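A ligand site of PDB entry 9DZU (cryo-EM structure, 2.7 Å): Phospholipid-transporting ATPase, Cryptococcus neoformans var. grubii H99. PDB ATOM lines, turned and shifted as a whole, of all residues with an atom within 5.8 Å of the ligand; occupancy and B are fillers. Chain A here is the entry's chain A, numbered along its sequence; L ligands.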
ATOM      1  N   LEU A 123      27.500   0.068  11.021  1.00  0.00           N
ATOM      2  CA  LEU A 123      27.270  -0.179  12.446  1.00  0.00           C
ATOM      3  C   LEU A 123      26.357  -1.381  12.658  1.00  0.00           C
ATOM      4  O   LEU A 123      26.410  -2.006  13.723  1.00  0.00           O
ATOM      5  CB  LEU A 123      26.671   1.071  13.095  1.00  0.00           C
ATOM      6  CG  LEU A 123      26.659   1.100  14.620  1.00  0.00           C
ATOM      7  CD1 LEU A 123      28.066   0.941  15.168  1.00  0.00           C
ATOM      8  CD2 LEU A 123      26.027   2.374  15.130  1.00  0.00           C
ATOM      9  N   VAL A 124      25.532  -1.721  11.668  1.00  0.00           N
ATOM     10  CA  VAL A 124      24.731  -2.942  11.756  1.00  0.00           C
ATOM     11  C   VAL A 124      25.614  -4.165  11.609  1.00  0.00           C
ATOM     12  O   VAL A 124      25.441  -5.170  12.320  1.00  0.00           O
ATOM     13  CB  VAL A 124      23.605  -2.906  10.712  1.00  0.00           C
ATOM     14  CG1 VAL A 124      22.952  -4.277  10.603  1.00  0.00           C
ATOM     15  CG2 VAL A 124      22.563  -1.866  11.087  1.00  0.00           C
ATOM     16  N   LEU A 126      28.827  -4.256  12.250  1.00  0.00           N
ATOM     17  CA  LEU A 126      29.903  -4.256  13.238  1.00  0.00           C
ATOM     18  C   LEU A 126      29.753  -5.321  14.319  1.00  0.00           C
ATOM     19  O   LEU A 126      30.759  -5.990  14.633  1.00  0.00           O
ATOM     20  CB  LEU A 126      30.035  -2.858  13.849  1.00  0.00           C
ATOM     21  CG  LEU A 126      31.285  -2.512  14.656  1.00  0.00           C
ATOM     22  CD1 LEU A 126      31.142  -2.897  16.136  1.00  0.00           C
ATOM     23  CD2 LEU A 126      32.528  -3.167  14.054  1.00  0.00           C
ATOM     24  N   PRO A 127      28.585  -5.513  14.947  1.00  0.00           N
ATOM     25  CA  PRO A 127      28.510  -6.564  15.986  1.00  0.00           C
ATOM     26  C   PRO A 127      28.816  -7.958  15.469  1.00  0.00           C
ATOM     27  O   PRO A 127      29.527  -8.717  16.135  1.00  0.00           O
ATOM     28  CB  PRO A 127      27.059  -6.459  16.486  1.00  0.00           C
ATOM     29  CG  PRO A 127      26.632  -5.093  16.120  1.00  0.00           C
ATOM     30  CD  PRO A 127      27.321  -4.781  14.838  1.00  0.00           C
ATOM     31  N   ILE A 130      32.478  -8.277  14.908  1.00  0.00           N
ATOM     32  CA  ILE A 130      33.175  -8.402  16.189  1.00  0.00           C
ATOM     33  C   ILE A 130      33.058  -9.828  16.729  1.00  0.00           C
ATOM     34  O   ILE A 130      34.050 -10.402  17.207  1.00  0.00           O
ATOM     35  CB  ILE A 130      32.648  -7.370  17.197  1.00  0.00           C
ATOM     36  CG1 ILE A 130      33.115  -5.966  16.807  1.00  0.00           C
ATOM     37  CG2 ILE A 130      33.114  -7.705  18.599  1.00  0.00           C
ATOM     38  CD1 ILE A 130      34.624  -5.817  16.764  1.00  0.00           C
ATOM     39  N   VAL A 131      31.868 -10.417  16.660  1.00  0.00           N
ATOM     40  CA  VAL A 131      31.698 -11.796  17.124  1.00  0.00           C
ATOM     41  C   VAL A 131      32.588 -12.730  16.317  1.00  0.00           C
ATOM     42  O   VAL A 131      33.315 -13.570  16.886  1.00  0.00           O
ATOM     43  CB  VAL A 131      30.215 -12.218  17.022  1.00  0.00           C
ATOM     44  CG1 VAL A 131      30.053 -13.657  17.465  1.00  0.00           C
ATOM     45  CG2 VAL A 131      29.343 -11.308  17.839  1.00  0.00           C
ATOM     46  N   ILE A 134      36.323 -12.190  17.183  1.00  0.00           N
ATOM     47  CA  ILE A 134      36.717 -12.683  18.493  1.00  0.00           C
ATOM     48  C   ILE A 134      36.805 -14.206  18.494  1.00  0.00           C
ATOM     49  O   ILE A 134      37.767 -14.780  19.008  1.00  0.00           O
ATOM     50  CB  ILE A 134      35.730 -12.174  19.565  1.00  0.00           C
ATOM     51  CG1 ILE A 134      35.965 -10.695  19.829  1.00  0.00           C
ATOM     52  CG2 ILE A 134      35.880 -12.981  20.855  1.00  0.00           C
ATOM     53  CD1 ILE A 134      35.179 -10.152  20.987  1.00  0.00           C
ATOM     54  N   GLN A 476      14.761  -8.489  17.120  1.00  0.00           N
ATOM     55  CA  GLN A 476      15.955  -9.284  16.896  1.00  0.00           C
ATOM     56  C   GLN A 476      16.670  -9.637  18.185  1.00  0.00           C
ATOM     57  O   GLN A 476      17.493 -10.564  18.181  1.00  0.00           O
ATOM     58  CB  GLN A 476      16.907  -8.547  15.954  1.00  0.00           C
ATOM     59  CG  GLN A 476      17.380  -7.204  16.477  1.00  0.00           C
ATOM     60  CD  GLN A 476      18.323  -6.515  15.523  1.00  0.00           C
ATOM     61  OE1 GLN A 476      18.993  -7.162  14.725  1.00  0.00           O
ATOM     62  NE2 GLN A 476      18.376  -5.188  15.607  1.00  0.00           N
ATOM     63  N   ASN A 477      16.388  -8.935  19.285  1.00  0.00           N
ATOM     64  CA  ASN A 477      17.032  -9.230  20.549  1.00  0.00           C
ATOM     65  C   ASN A 477      16.471 -10.477  21.222  1.00  0.00           C
ATOM     66  O   ASN A 477      17.030 -10.903  22.238  1.00  0.00           O
ATOM     67  CB  ASN A 477      16.908  -8.036  21.497  1.00  0.00           C
ATOM     68  CG  ASN A 477      17.818  -6.892  21.115  1.00  0.00           C
ATOM     69  OD1 ASN A 477      18.353  -6.867  20.008  1.00  0.00           O
ATOM     70  ND2 ASN A 477      17.994  -5.952  22.027  1.00  0.00           N
ATOM     71  N   PRO A 480      19.779 -12.544  21.183  1.00  0.00           N
ATOM     72  CA  PRO A 480      20.783 -11.476  21.173  1.00  0.00           C
ATOM     73  C   PRO A 480      22.110 -11.935  20.590  1.00  0.00           C
ATOM     74  O   PRO A 480      22.481 -13.109  20.680  1.00  0.00           O
ATOM     75  CB  PRO A 480      20.928 -11.117  22.658  1.00  0.00           C
ATOM     76  CG  PRO A 480      20.547 -12.364  23.373  1.00  0.00           C
ATOM     77  CD  PRO A 480      19.459 -12.994  22.554  1.00  0.00           C
ATOM     78  N   ILE A 481      22.823 -10.982  19.985  1.00  0.00           N
ATOM     79  CA  ILE A 481      24.155 -11.276  19.470  1.00  0.00           C
ATOM     80  C   ILE A 481      25.217 -11.112  20.541  1.00  0.00           C
ATOM     81  O   ILE A 481      26.267 -11.754  20.462  1.00  0.00           O
ATOM     82  CB  ILE A 481      24.448 -10.391  18.237  1.00  0.00           C
ATOM     83  CG1 ILE A 481      25.754 -10.802  17.565  1.00  0.00           C
ATOM     84  CG2 ILE A 481      24.487  -8.929  18.630  1.00  0.00           C
ATOM     85  CD1 ILE A 481      26.053 -10.047  16.295  1.00  0.00           C
ATOM     86  N   SER A 482      24.965 -10.276  21.550  1.00  0.00           N
ATOM     87  CA  SER A 482      25.894 -10.125  22.661  1.00  0.00           C
ATOM     88  C   SER A 482      25.977 -11.358  23.552  1.00  0.00           C
ATOM     89  O   SER A 482      26.901 -11.453  24.367  1.00  0.00           O
ATOM     90  CB  SER A 482      25.501  -8.918  23.517  1.00  0.00           C
ATOM     91  OG  SER A 482      24.163  -9.021  23.957  1.00  0.00           O
ATOM     92  N   LEU A 483      25.029 -12.293  23.413  1.00  0.00           N
ATOM     93  CA  LEU A 483      25.058 -13.506  24.222  1.00  0.00           C
ATOM     94  C   LEU A 483      26.304 -14.322  23.953  1.00  0.00           C
ATOM     95  O   LEU A 483      26.972 -14.783  24.883  1.00  0.00           O
ATOM     96  CB  LEU A 483      23.798 -14.320  23.963  1.00  0.00           C
ATOM     97  CG  LEU A 483      23.691 -15.723  24.563  1.00  0.00           C
ATOM     98  CD1 LEU A 483      22.321 -15.909  25.188  1.00  0.00           C
ATOM     99  CD2 LEU A 483      23.923 -16.779  23.502  1.00  0.00           C
ATOM    100  N   ILE A 485      29.245 -13.446  22.491  1.00  0.00           N
ATOM    101  CA  ILE A 485      30.480 -12.776  22.882  1.00  0.00           C
ATOM    102  C   ILE A 485      30.715 -12.928  24.373  1.00  0.00           C
ATOM    103  O   ILE A 485      31.818 -13.267  24.823  1.00  0.00           O
ATOM    104  CB  ILE A 485      30.433 -11.283  22.485  1.00  0.00           C
ATOM    105  CG1 ILE A 485      29.432 -11.068  21.362  1.00  0.00           C
ATOM    106  CG2 ILE A 485      31.808 -10.810  22.069  1.00  0.00           C
ATOM    107  CD1 ILE A 485      29.287  -9.623  20.964  1.00  0.00           C
ATOM    108  N   SER A 486      29.665 -12.704  25.171  1.00  0.00           N
ATOM    109  CA  SER A 486      29.787 -12.850  26.616  1.00  0.00           C
ATOM    110  C   SER A 486      30.109 -14.284  27.006  1.00  0.00           C
ATOM    111  O   SER A 486      30.928 -14.529  27.891  1.00  0.00           O
ATOM    112  CB  SER A 486      28.499 -12.384  27.293  1.00  0.00           C
ATOM    113  OG  SER A 486      28.162 -11.071  26.895  1.00  0.00           O
ATOM    114  N   ALA A 489      33.817 -14.966  26.180  1.00  0.00           N
ATOM    115  CA  ALA A 489      34.711 -14.307  27.128  1.00  0.00           C
ATOM    116  C   ALA A 489      34.682 -14.995  28.485  1.00  0.00           C
ATOM    117  O   ALA A 489      35.728 -15.196  29.108  1.00  0.00           O
ATOM    118  CB  ALA A 489      34.328 -12.836  27.266  1.00  0.00           C
ATOM    119  N   VAL A 490      33.491 -15.369  28.955  1.00  0.00           N
ATOM    120  CA  VAL A 490      33.369 -16.031  30.244  1.00  0.00           C
ATOM    121  C   VAL A 490      34.071 -17.391  30.214  1.00  0.00           C
ATOM    122  O   VAL A 490      34.755 -17.758  31.178  1.00  0.00           O
ATOM    123  CB  VAL A 490      31.888 -16.156  30.635  1.00  0.00           C
ATOM    124  CG1 VAL A 490      31.714 -17.189  31.738  1.00  0.00           C
ATOM    125  CG2 VAL A 490      31.367 -14.808  31.092  1.00  0.00           C
ATOM    126  N   ILE A 493      37.819 -16.839  30.394  1.00  0.00           N
ATOM    127  CA  ILE A 493      38.260 -16.495  31.745  1.00  0.00           C
ATOM    128  C   ILE A 493      38.153 -17.696  32.682  1.00  0.00           C
ATOM    129  O   ILE A 493      38.950 -17.827  33.607  1.00  0.00           O
ATOM    130  CB  ILE A 493      37.478 -15.276  32.261  1.00  0.00           C
ATOM    131  CG1 ILE A 493      37.711 -14.082  31.342  1.00  0.00           C
ATOM    132  CG2 ILE A 493      37.899 -14.923  33.673  1.00  0.00           C
ATOM    133  CD1 ILE A 493      37.025 -12.815  31.796  1.00  0.00           C
ATOM    134  N   LEU A1106      19.087   0.354  21.829  1.00  0.00           N
ATOM    135  CA  LEU A1106      20.409   0.132  21.253  1.00  0.00           C
ATOM    136  C   LEU A1106      21.423  -0.246  22.324  1.00  0.00           C
ATOM    137  O   LEU A1106      22.306  -1.079  22.082  1.00  0.00           O
ATOM    138  CB  LEU A1106      20.858   1.373  20.489  1.00  0.00           C
ATOM    139  CG  LEU A1106      22.208   1.338  19.782  1.00  0.00           C
ATOM    140  CD1 LEU A1106      22.217   0.270  18.707  1.00  0.00           C
ATOM    141  CD2 LEU A1106      22.518   2.695  19.199  1.00  0.00           C
ATOM    142  N   ASN A1109      21.997  -4.147  25.847  1.00  0.00           N
ATOM    143  CA  ASN A1109      23.010  -5.133  26.222  1.00  0.00           C
ATOM    144  C   ASN A1109      24.392  -4.533  26.380  1.00  0.00           C
ATOM    145  O   ASN A1109      25.210  -5.088  27.126  1.00  0.00           O
ATOM    146  CB  ASN A1109      23.066  -6.253  25.179  1.00  0.00           C
ATOM    147  CG  ASN A1109      21.725  -6.924  24.973  1.00  0.00           C
ATOM    148  OD1 ASN A1109      21.359  -7.834  25.701  1.00  0.00           O
ATOM    149  ND2 ASN A1109      20.984  -6.461  23.974  1.00  0.00           N
ATOM    150  N   VAL A1110      24.681  -3.423  25.708  1.00  0.00           N
ATOM    151  CA  VAL A1110      25.997  -2.802  25.814  1.00  0.00           C
ATOM    152  C   VAL A1110      26.201  -2.214  27.204  1.00  0.00           C
ATOM    153  O   VAL A1110      27.250  -2.413  27.817  1.00  0.00           O
ATOM    154  CB  VAL A1110      26.179  -1.749  24.717  1.00  0.00           C
ATOM    155  CG1 VAL A1110      27.646  -1.381  24.573  1.00  0.00           C
ATOM    156  CG2 VAL A1110      25.617  -2.241  23.400  1.00  0.00           C
ATOM    157  N   LEU A1114      24.747  -5.709  31.249  1.00  0.00           N
ATOM    158  CA  LEU A1114      25.881  -6.545  30.887  1.00  0.00           C
ATOM    159  C   LEU A1114      26.643  -7.070  32.098  1.00  0.00           C
ATOM    160  O   LEU A1114      27.066  -8.237  32.117  1.00  0.00           O
ATOM    161  CB  LEU A1114      26.829  -5.756  29.976  1.00  0.00           C
ATOM    162  CG  LEU A1114      28.168  -6.394  29.610  1.00  0.00           C
ATOM    163  CD1 LEU A1114      27.957  -7.634  28.752  1.00  0.00           C
ATOM    164  CD2 LEU A1114      29.065  -5.382  28.913  1.00  0.00           C
ATOM    165  N   ILE A1118      27.816 -10.833  33.431  1.00  0.00           N
ATOM    166  CA  ILE A1118      29.229 -11.175  33.491  1.00  0.00           C
ATOM    167  C   ILE A1118      29.614 -11.637  34.889  1.00  0.00           C
ATOM    168  O   ILE A1118      30.374 -12.594  35.064  1.00  0.00           O
ATOM    169  CB  ILE A1118      30.089  -9.981  33.023  1.00  0.00           C
ATOM    170  CG1 ILE A1118      29.825  -9.708  31.540  1.00  0.00           C
ATOM    171  CG2 ILE A1118      31.556 -10.247  33.259  1.00  0.00           C
ATOM    172  CD1 ILE A1118      29.894 -10.937  30.666  1.00  0.00           C
ATOM    173  N   LEU A1122      31.124 -15.299  35.914  1.00  0.00           N
ATOM    174  CA  LEU A1122      32.522 -15.370  36.363  1.00  0.00           C
ATOM    175  C   LEU A1122      32.676 -15.663  37.848  1.00  0.00           C
ATOM    176  O   LEU A1122      33.503 -16.506  38.220  1.00  0.00           O
ATOM    177  CB  LEU A1122      33.240 -14.063  36.023  1.00  0.00           C
ATOM    178  CG  LEU A1122      33.476 -13.768  34.547  1.00  0.00           C
ATOM    179  CD1 LEU A1122      34.343 -12.542  34.392  1.00  0.00           C
ATOM    180  CD2 LEU A1122      34.116 -14.955  33.868  1.00  0.00           C
HETATM  181  C1  LIG L   1      36.518  -9.837  29.037  1.00  0.00           C
HETATM  182  C2  LIG L   1      35.739  -9.463  30.307  1.00  0.00           C
HETATM  183  C3  LIG L   1      36.676  -9.601  31.515  1.00  0.00           C
HETATM  184  C4  LIG L   1      35.331  -7.973  30.297  1.00  0.00           C
HETATM  185  C5  LIG L   1      34.517 -10.390  30.494  1.00  0.00           C
HETATM  186  C6  LIG L   1      33.378 -10.353  29.511  1.00  0.00           C
HETATM  187  C7  LIG L   1      33.248  -9.500  28.508  1.00  0.00           C
HETATM  188  C8  LIG L   1      32.494  -9.641  27.294  1.00  0.00           C
HETATM  189  C9  LIG L   1      32.509  -8.671  26.402  1.00  0.00           C
HETATM  190  C10 LIG L   1      33.677  -8.371  25.512  1.00  0.00           C
HETATM  191  C11 LIG L   1      34.974  -9.209  25.534  1.00  0.00           C
HETATM  192  C12 LIG L   1      35.888  -8.680  24.425  1.00  0.00           C
HETATM  193  C13 LIG L   1      35.189  -7.411  23.911  1.00  0.00           C
HETATM  194  C14 LIG L   1      34.432  -7.299  22.834  1.00  0.00           C
HETATM  195  C15 LIG L   1      33.747  -6.112  22.358  1.00  0.00           C
HETATM  196  C16 LIG L   1      32.489  -6.411  21.999  1.00  0.00           C
HETATM  197  C17 LIG L   1      31.365  -5.513  21.444  1.00  0.00           C
HETATM  198  C18 LIG L   1      30.043  -6.153  21.857  1.00  0.00           C
HETATM  199  C19 LIG L   1      30.162  -6.303  23.385  1.00  0.00           C
HETATM  200  C20 LIG L   1      28.779  -5.340  21.544  1.00  0.00           C
HETATM  201  C21 LIG L   1      27.580  -5.857  22.338  1.00  0.00           C
HETATM  202  C22 LIG L   1      26.208  -5.397  21.830  1.00  0.00           C
HETATM  203  C23 LIG L   1      25.648  -6.185  20.639  1.00  0.00           C
HETATM  204  C24 LIG L   1      24.175  -6.665  20.768  1.00  0.00           C
HETATM  205  O1  LIG L   1      22.137  -6.470  19.470  1.00  0.00           O
HETATM  206  O2  LIG L   1      23.438  -5.281  16.421  1.00  0.00           O
HETATM  207  O3  LIG L   1      24.440  -3.773  19.032  1.00  0.00           O
HETATM  208  O4  LIG L   1      21.659  -7.223  17.447  1.00  0.00           O
HETATM  209  O5  LIG L   1      23.705  -6.767  22.084  1.00  0.00           O
HETATM  210  O6  LIG L   1      28.511  -5.352  20.178  1.00  0.00           O
HETATM  211  O7  LIG L   1      27.592  -7.247  22.266  1.00  0.00           O
HETATM  212  O8  LIG L   1      25.354  -5.455  22.928  1.00  0.00           O
HETATM  213  O9  LIG L   1      26.420  -7.320  20.464  1.00  0.00           O
HETATM  214  C25 LIG L   1      23.281  -5.720  20.004  1.00  0.00           C
HETATM  215  C26 LIG L   1      22.158  -6.396  18.138  1.00  0.00           C
HETATM  216  C27 LIG L   1      22.908  -5.154  17.728  1.00  0.00           C
HETATM  217  C28 LIG L   1      24.012  -5.141  18.788  1.00  0.00           C
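An oxygen (O9) of the ligand sits at hydrogen-bond distance from the backbone NH of Ser 482 (3.5 Å).
An oxygen (O5) of the ligand is in hydrogen-bond range of the side-chain hydroxyl (OG) of Ser 482, at 3.0 Å.
O5 of the ligand lies close to ND2 of Asn 1109 (3.3 Å).
OG of Ser 486 is in hydrogen-bond range of O of Ser 482.
Residues that only touch the ligand: Ile 481, Ile 485, Pro 127, Ile 493, Val 1110, Ala 489, Ile 134, Ile 130, Ile 1118, Gln 476 and Asn 477.
Hydrophobic or aromatic side chains that line the ligand: Pro 127, Ile 130, Ile 134, Ile 481, Ile 485, Ala 489, Ile 493, Val 1110 and Ile 1118.
The nearest printed residue that does not touch the ligand is Ser 486 (4.3 Å).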
